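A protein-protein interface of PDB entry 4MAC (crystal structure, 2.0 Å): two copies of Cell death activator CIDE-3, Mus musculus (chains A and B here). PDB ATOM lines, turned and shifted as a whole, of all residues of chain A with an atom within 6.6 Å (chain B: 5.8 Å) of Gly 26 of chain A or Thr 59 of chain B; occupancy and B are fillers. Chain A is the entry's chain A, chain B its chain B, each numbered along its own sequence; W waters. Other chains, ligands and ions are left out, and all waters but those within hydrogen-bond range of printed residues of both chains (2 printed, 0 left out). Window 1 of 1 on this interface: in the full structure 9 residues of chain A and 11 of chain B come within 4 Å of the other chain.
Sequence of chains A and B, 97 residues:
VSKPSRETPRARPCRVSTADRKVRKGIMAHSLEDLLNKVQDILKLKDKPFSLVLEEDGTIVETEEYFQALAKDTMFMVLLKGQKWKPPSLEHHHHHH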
ATOM      1  N   PRO A  13     -29.385  19.833  -2.423  1.00  0.00           N
ATOM      2  CA  PRO A  13     -29.039  19.150  -3.663  1.00  0.00           C
ATOM      3  C   PRO A  13     -30.251  18.860  -4.583  1.00  0.00           C
ATOM      4  O   PRO A  13     -31.234  18.262  -4.131  1.00  0.00           O
ATOM      5  CB  PRO A  13     -28.388  17.840  -3.178  1.00  0.00           C
ATOM      6  CG  PRO A  13     -28.964  17.590  -1.880  1.00  0.00           C
ATOM      7  CD  PRO A  13     -29.163  18.957  -1.254  1.00  0.00           C
ATOM      8  N   CYS A  14     -30.142  19.238  -5.862  1.00  0.00           N
ATOM      9  CA  CYS A  14     -31.228  19.073  -6.841  1.00  0.00           C
ATOM     10  C   CYS A  14     -30.643  18.308  -7.997  1.00  0.00           C
ATOM     11  O   CYS A  14     -29.507  18.610  -8.397  1.00  0.00           O
ATOM     12  CB  CYS A  14     -31.722  20.434  -7.345  1.00  0.00           C
ATOM     13  SG  CYS A  14     -32.172  21.548  -5.999  1.00  0.00           S
ATOM     14  N   ARG A  15     -31.409  17.341  -8.519  1.00  0.00           N
ATOM     15  CA  ARG A  15     -31.012  16.597  -9.690  1.00  0.00           C
ATOM     16  C   ARG A  15     -31.801  17.244 -10.789  1.00  0.00           C
ATOM     17  O   ARG A  15     -32.999  17.348 -10.684  1.00  0.00           O
ATOM     18  CB  ARG A  15     -31.415  15.128  -9.537  1.00  0.00           C
ATOM     19  CG  ARG A  15     -30.862  14.508  -8.238  1.00  0.00           C
ATOM     20  CD  ARG A  15     -31.018  13.016  -8.210  1.00  0.00           C
ATOM     21  NE  ARG A  15     -30.508  12.494  -6.925  1.00  0.00           N
ATOM     22  CZ  ARG A  15     -30.541  11.214  -6.568  1.00  0.00           C
ATOM     23  NH1 ARG A  15     -31.025  10.276  -7.417  1.00  0.00           N
ATOM     24  NH2 ARG A  15     -30.056  10.879  -5.369  1.00  0.00           N
ATOM     25  N   VAL A  16     -31.133  17.676 -11.853  1.00  0.00           N
ATOM     26  CA  VAL A  16     -31.852  18.465 -12.872  1.00  0.00           C
ATOM     27  C   VAL A  16     -31.532  17.991 -14.291  1.00  0.00           C
ATOM     28  O   VAL A  16     -30.357  17.932 -14.703  1.00  0.00           O
ATOM     29  CB  VAL A  16     -31.523  20.001 -12.750  1.00  0.00           C
ATOM     30  CG1 VAL A  16     -32.432  20.812 -13.640  1.00  0.00           C
ATOM     31  CG2 VAL A  16     -31.583  20.535 -11.274  1.00  0.00           C
ATOM     32  N   ARG A  24     -28.037  15.437 -17.317  1.00  0.00           N
ATOM     33  CA  ARG A  24     -28.619  15.433 -16.002  1.00  0.00           C
ATOM     34  C   ARG A  24     -27.518  15.796 -15.023  1.00  0.00           C
ATOM     35  O   ARG A  24     -26.441  15.204 -15.061  1.00  0.00           O
ATOM     36  CB  ARG A  24     -29.184  14.037 -15.703  1.00  0.00           C
ATOM     37  CG  ARG A  24     -30.685  14.010 -15.544  1.00  0.00           C
ATOM     38  CD  ARG A  24     -31.378  12.790 -16.193  1.00  0.00           C
ATOM     39  NE  ARG A  24     -30.546  11.596 -16.235  1.00  0.00           N
ATOM     40  CZ  ARG A  24     -30.121  10.995 -17.348  1.00  0.00           C
ATOM     41  NH1 ARG A  24     -30.432  11.461 -18.539  1.00  0.00           N
ATOM     42  NH2 ARG A  24     -29.372   9.895 -17.266  1.00  0.00           N
ATOM     43  N   LYS A  25     -27.753  16.796 -14.170  1.00  0.00           N
ATOM     44  CA  LYS A  25     -26.680  17.235 -13.305  1.00  0.00           C
ATOM     45  C   LYS A  25     -27.138  17.611 -11.913  1.00  0.00           C
ATOM     46  O   LYS A  25     -28.220  18.151 -11.755  1.00  0.00           O
ATOM     47  CB  LYS A  25     -25.942  18.438 -13.937  1.00  0.00           C
ATOM     48  CG  LYS A  25     -25.271  18.124 -15.323  1.00  0.00           C
ATOM     49  CD  LYS A  25     -24.399  19.295 -15.682  1.00  0.00           C
ATOM     50  CE  LYS A  25     -23.536  19.063 -16.935  1.00  0.00           C
ATOM     51  NZ  LYS A  25     -22.654  20.260 -17.070  1.00  0.00           N
ATOM     52  N   GLY A  26     -26.272  17.372 -10.925  1.00  0.00           N
ATOM     53  CA  GLY A  26     -26.536  17.731  -9.527  1.00  0.00           C
ATOM     54  C   GLY A  26     -26.177  19.187  -9.259  1.00  0.00           C
ATOM     55  O   GLY A  26     -25.054  19.590  -9.522  1.00  0.00           O
ATOM     56  N   ILE A  27     -27.137  19.991  -8.802  1.00  0.00           N
ATOM     57  CA  ILE A  27     -26.902  21.411  -8.624  1.00  0.00           C
ATOM     58  C   ILE A  27     -27.301  21.740  -7.210  1.00  0.00           C
ATOM     59  O   ILE A  27     -28.336  21.251  -6.738  1.00  0.00           O
ATOM     60  CB  ILE A  27     -27.786  22.262  -9.580  1.00  0.00           C
ATOM     61  CG1 ILE A  27     -27.515  21.893 -11.047  1.00  0.00           C
ATOM     62  CG2 ILE A  27     -27.615  23.781  -9.302  1.00  0.00           C
ATOM     63  CD1 ILE A  27     -28.326  22.633 -12.080  1.00  0.00           C
ATOM     64  N   MET A  28     -26.491  22.548  -6.533  1.00  0.00           N
ATOM     65  CA  MET A  28     -26.824  22.974  -5.181  1.00  0.00           C
ATOM     66  C   MET A  28     -27.673  24.243  -5.210  1.00  0.00           C
ATOM     67  O   MET A  28     -27.355  25.154  -5.947  1.00  0.00           O
ATOM     68  CB  MET A  28     -25.514  23.197  -4.391  1.00  0.00           C
ATOM     69  CG  MET A  28     -24.744  21.882  -4.102  1.00  0.00           C
ATOM     70  SD  MET A  28     -25.740  20.633  -3.244  1.00  0.00           S
ATOM     71  CE  MET A  28     -26.120  21.466  -1.698  1.00  0.00           C
ATOM     72  N   ILE A  42     -25.098  25.875 -16.058  1.00  0.00           N
ATOM     73  CA  ILE A  42     -24.744  24.499 -15.639  1.00  0.00           C
ATOM     74  C   ILE A  42     -25.108  23.445 -16.679  1.00  0.00           C
ATOM     75  O   ILE A  42     -24.317  22.566 -16.993  1.00  0.00           O
ATOM     76  CB  ILE A  42     -25.286  24.175 -14.247  1.00  0.00           C
ATOM     77  CG1 ILE A  42     -24.591  25.101 -13.218  1.00  0.00           C
ATOM     78  CG2 ILE A  42     -25.058  22.651 -13.906  1.00  0.00           C
ATOM     79  CD1 ILE A  42     -25.032  24.944 -11.748  1.00  0.00           C
ATOM     80  N   MET A  75     -36.048  14.105  -9.480  1.00  0.00           N
ATOM     81  CA  MET A  75     -35.475  14.578 -10.739  1.00  0.00           C
ATOM     82  C   MET A  75     -36.315  15.710 -11.339  1.00  0.00           C
ATOM     83  O   MET A  75     -37.490  15.518 -11.615  1.00  0.00           O
ATOM     84  CB  MET A  75     -35.301  13.414 -11.726  1.00  0.00           C
ATOM     85  CG  MET A  75     -34.803  13.855 -13.114  1.00  0.00           C
ATOM     86  SD  MET A  75     -33.092  14.343 -13.092  1.00  0.00           S
ATOM     87  CE  MET A  75     -32.309  12.854 -12.355  1.00  0.00           C
ATOM     88  N   LEU B  52     -18.074  11.166 -12.922  1.00  0.00           N
ATOM     89  CA  LEU B  52     -18.656  10.479 -11.806  1.00  0.00           C
ATOM     90  C   LEU B  52     -20.125  10.804 -11.842  1.00  0.00           C
ATOM     91  O   LEU B  52     -20.524  11.968 -11.879  1.00  0.00           O
ATOM     92  CB  LEU B  52     -18.088  10.988 -10.489  1.00  0.00           C
ATOM     93  CG  LEU B  52     -18.536  10.134  -9.295  1.00  0.00           C
ATOM     94  CD1 LEU B  52     -18.000   8.627  -9.391  1.00  0.00           C
ATOM     95  CD2 LEU B  52     -18.212  10.772  -7.940  1.00  0.00           C
ATOM     96  N   VAL B  53     -20.935   9.764 -11.791  1.00  0.00           N
ATOM     97  CA  VAL B  53     -22.352   9.955 -11.949  1.00  0.00           C
ATOM     98  C   VAL B  53     -23.121   9.156 -10.884  1.00  0.00           C
ATOM     99  O   VAL B  53     -22.545   8.271 -10.254  1.00  0.00           O
ATOM    100  CB  VAL B  53     -22.580   9.442 -13.368  1.00  0.00           C
ATOM    101  CG1 VAL B  53     -23.140   8.048 -13.426  1.00  0.00           C
ATOM    102  CG2 VAL B  53     -23.143  10.427 -14.246  1.00  0.00           C
ATOM    103  N   LEU B  54     -24.410   9.460 -10.666  1.00  0.00           N
ATOM    104  CA  LEU B  54     -25.210   8.666  -9.753  1.00  0.00           C
ATOM    105  C   LEU B  54     -25.601   7.410 -10.424  1.00  0.00           C
ATOM    106  O   LEU B  54     -26.178   7.422 -11.547  1.00  0.00           O
ATOM    107  CB  LEU B  54     -26.461   9.392  -9.248  1.00  0.00           C
ATOM    108  CG  LEU B  54     -26.149  10.666  -8.444  1.00  0.00           C
ATOM    109  CD1 LEU B  54     -27.369  11.295  -7.825  1.00  0.00           C
ATOM    110  CD2 LEU B  54     -25.245  10.251  -7.322  1.00  0.00           C
ATOM    111  N   ASP B  57     -29.603   7.048 -11.547  1.00  0.00           N
ATOM    112  CA  ASP B  57     -30.225   7.812 -12.648  1.00  0.00           C
ATOM    113  C   ASP B  57     -29.261   8.616 -13.552  1.00  0.00           C
ATOM    114  O   ASP B  57     -29.697   9.321 -14.497  1.00  0.00           O
ATOM    115  CB  ASP B  57     -31.351   8.735 -12.083  1.00  0.00           C
ATOM    116  CG  ASP B  57     -30.821   9.752 -11.076  1.00  0.00           C
ATOM    117  OD1 ASP B  57     -29.654  10.133 -11.202  1.00  0.00           O
ATOM    118  OD2 ASP B  57     -31.536  10.244 -10.193  1.00  0.00           O
ATOM    119  N   GLY B  58     -27.954   8.524 -13.299  1.00  0.00           N
ATOM    120  CA  GLY B  58     -26.987   9.164 -14.209  1.00  0.00           C
ATOM    121  C   GLY B  58     -26.823  10.670 -14.004  1.00  0.00           C
ATOM    122  O   GLY B  58     -26.233  11.348 -14.813  1.00  0.00           O
ATOM    123  N   THR B  59     -27.299  11.186 -12.886  1.00  0.00           N
ATOM    124  CA  THR B  59     -27.010  12.595 -12.539  1.00  0.00           C
ATOM    125  C   THR B  59     -25.507  12.811 -12.367  1.00  0.00           C
ATOM    126  O   THR B  59     -24.852  12.065 -11.633  1.00  0.00           O
ATOM    127  CB  THR B  59     -27.692  12.941 -11.228  1.00  0.00           C
ATOM    128  OG1 THR B  59     -29.086  12.652 -11.341  1.00  0.00           O
ATOM    129  CG2 THR B  59     -27.486  14.377 -10.857  1.00  0.00           C
ATOM    130  N   ILE B  60     -24.969  13.848 -12.999  1.00  0.00           N
ATOM    131  CA  ILE B  60     -23.537  14.051 -12.976  1.00  0.00           C
ATOM    132  C   ILE B  60     -23.163  14.793 -11.706  1.00  0.00           C
ATOM    133  O   ILE B  60     -23.777  15.819 -11.353  1.00  0.00           O
ATOM    134  CB  ILE B  60     -23.081  14.803 -14.203  1.00  0.00           C
ATOM    135  CG1 ILE B  60     -23.328  13.938 -15.433  1.00  0.00           C
ATOM    136  CG2 ILE B  60     -21.570  15.159 -14.129  1.00  0.00           C
ATOM    137  CD1 ILE B  60     -23.550  14.788 -16.692  1.00  0.00           C
ATOM    138  N   VAL B  61     -22.184  14.246 -11.013  1.00  0.00           N
ATOM    139  CA  VAL B  61     -21.652  14.822  -9.805  1.00  0.00           C
ATOM    140  C   VAL B  61     -20.407  15.593 -10.223  1.00  0.00           C
ATOM    141  O   VAL B  61     -19.380  14.995 -10.583  1.00  0.00           O
ATOM    142  CB  VAL B  61     -21.188  13.762  -8.847  1.00  0.00           C
ATOM    143  CG1 VAL B  61     -20.761  14.420  -7.513  1.00  0.00           C
ATOM    144  CG2 VAL B  61     -22.299  12.732  -8.616  1.00  0.00           C
ATOM    145  N   GLU B  62     -20.507  16.906 -10.249  1.00  0.00           N
ATOM    146  CA  GLU B  62     -19.364  17.657 -10.744  1.00  0.00           C
ATOM    147  C   GLU B  62     -18.931  18.770  -9.849  1.00  0.00           C
ATOM    148  O   GLU B  62     -17.999  19.533 -10.186  1.00  0.00           O
ATOM    149  CB  GLU B  62     -19.557  18.172 -12.169  1.00  0.00           C
ATOM    150  CG  GLU B  62     -20.726  19.089 -12.360  1.00  0.00           C
ATOM    151  CD  GLU B  62     -20.859  19.446 -13.838  1.00  0.00           C
ATOM    152  OE1 GLU B  62     -20.278  18.731 -14.701  1.00  0.00           O
ATOM    153  OE2 GLU B  62     -21.526  20.446 -14.144  1.00  0.00           O
ATOM    154  N   THR B  63     -19.533  18.821  -8.683  1.00  0.00           N
ATOM    155  CA  THR B  63     -19.013  19.771  -7.722  1.00  0.00           C
ATOM    156  C   THR B  63     -18.788  19.132  -6.377  1.00  0.00           C
ATOM    157  O   THR B  63     -19.524  18.193  -5.942  1.00  0.00           O
ATOM    158  CB  THR B  63     -19.916  20.993  -7.586  1.00  0.00           C
ATOM    159  OG1 THR B  63     -19.318  21.859  -6.633  1.00  0.00           O
ATOM    160  CG2 THR B  63     -21.225  20.594  -7.015  1.00  0.00           C
ATOM    161  N   TYR B  66     -21.934  19.344  -3.985  1.00  0.00           N
ATOM    162  CA  TYR B  66     -22.923  18.339  -4.322  1.00  0.00           C
ATOM    163  C   TYR B  66     -22.444  16.933  -3.967  1.00  0.00           C
ATOM    164  O   TYR B  66     -23.227  16.116  -3.446  1.00  0.00           O
ATOM    165  CB  TYR B  66     -23.292  18.382  -5.785  1.00  0.00           C
ATOM    166  CG  TYR B  66     -24.484  17.474  -6.096  1.00  0.00           C
ATOM    167  CD1 TYR B  66     -25.799  17.892  -5.800  1.00  0.00           C
ATOM    168  CD2 TYR B  66     -24.292  16.231  -6.702  1.00  0.00           C
ATOM    169  CE1 TYR B  66     -26.883  17.086  -6.052  1.00  0.00           C
ATOM    170  CE2 TYR B  66     -25.369  15.410  -6.972  1.00  0.00           C
ATOM    171  CZ  TYR B  66     -26.654  15.846  -6.620  1.00  0.00           C
ATOM    172  OH  TYR B  66     -27.681  15.032  -6.890  1.00  0.00           O
HETATM  173  O   HOH W   1     -22.721  18.654  -9.178  1.00  0.00           O
HETATM  174  O   HOH W   2     -29.718  14.938  -5.077  1.00  0.00           O
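OD2 of Asp 57 of chain B is in salt-bridge range of NH1 of Arg 15 of chain A, 2.8 Å away.
The guanidinium group of Arg 24 of chain A lies within hydrogen-bond range of the backbone carbonyl oxygen of Asp 57 of chain B (2.8 Å).
The backbone carbonyl oxygen (O) of Arg 24 of chain A is in hydrogen-bond range of the backbone NH (N) of Ile 60 of chain B (2.9 Å).
The side-chain amino group (NZ) of Lys 25 of chain A lies within salt-bridge range of the side-chain carboxylate (OE2) of Glu 62 of chain B (3.1 Å).
N of Gly 26 of chain A is in hydrogen-bond range of O of Ile 60 of chain B, 3.0 Å away.
The backbone NH (N) of Ile 27 of chain A sits at hydrogen-bond distance from the backbone carbonyl oxygen (O) of Cys 14 of chain A, at 2.8 Å.
The backbone carbonyl oxygen (O) of Val 16 of chain A lies within hydrogen-bond range of the backbone NH (N) of Lys 25 of chain A, at 2.9 Å.
NZ of Lys 25 of chain A sits at hydrogen-bond distance from O of Ile 42 of chain A (2.8 Å).
N of Leu 54 of chain B is in hydrogen-bond range of O of Thr 59 of chain B (2.8 Å).
The side-chain carboxylate (OD1) of Asp 57 of chain B is in hydrogen-bond range of the side-chain hydroxyl (OG1) of Thr 59 of chain B (2.6 Å).
Among the printed residues, pairs that only touch across the chains: Pro 13 of chain A with Tyr 66 of chain B, Cys 14 of chain A with Tyr 66 of chain B, Arg 15 of chain A with Leu 54 of chain B, Arg 15 of chain A with Thr 59 of chain B, Arg 15 of chain A with Tyr 66 of chain B, Arg 24 of chain A with Gly 58 of chain B, Arg 24 of chain A with Thr 59 of chain B, Lys 25 of chain A with Thr 59 of chain B, Lys 25 of chain A with Ile 60 of chain B, Gly 26 of chain A with Thr 59 of chain B, Gly 26 of chain A with Tyr 66 of chain B, Ile 27 of chain A with Tyr 66 of chain B, Met 28 of chain A with Tyr 66 of chain B, Met 75 of chain A with Asp 57 of chain B and Met 75 of chain A with Thr 59 of chain B.
Gly 26 of chain A touches just these residues of chain B: Thr 59 (3.2 Å), Ile 60 (3.0 Å) and Tyr 66 (3.5 Å).
Thr 59 of chain B touches just these residues of chain A: Arg 15, Arg 24, Lys 25, Gly 26 and Met 75.
Printed residues of chain A within 4 Å of Asp 57 of chain B: Arg 15 (2.8 Å), Arg 24 (2.8 Å) and Met 75 (3.5 Å).
Printed residues of chain B within 4 Å of Pro 13 of chain A: Tyr 66.
Printed residues of chain A within 4 Å of Gly 58 of chain B: Arg 24.
Leu 52 of chain B touches none of the printed residues of chain A.
Val 16 of chain A touches none of the printed residues of chain B.
The nearest printed residue of chain B that does not touch Ile 27 of chain A is Ile 60 of chain B (5.9 Å).
Hydrophobic or aromatic side chains of chain A within 4 Å of the printed part of chain B: Pro 13, Met 28 and Met 75.
Along chain A the printed residues that touch a printed residue of chain B span positions 13 to 75.
Among the printed residues, 20 pairs touch across the chains.
Among the printed residues, Asp or Glu carboxylates within 4 Å of a Lys or Arg side-chain nitrogen of the other chain: Arg 15 of chain A with Asp 57 of chain B (2.8 Å) and Lys 25 of chain A with Glu 62 of chain B (3.1 Å).
No position is printed for both chains.
Of the 20 pairs that touch across the chains among the printed residues, none has its exchanged pair printed and touching as well.
Water W1 lies within hydrogen-bond range of the backbone carbonyl oxygen of Gly 26 of chain A (2.5 Å), the backbone NH of Glu 62 of chain B (3.0 Å) and the backbone NH of Thr 63 of chain B (3.2 Å).
Water W2 lies within hydrogen-bond range of OH of Tyr 66 of chain B and NE of Arg 15 of chain A.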
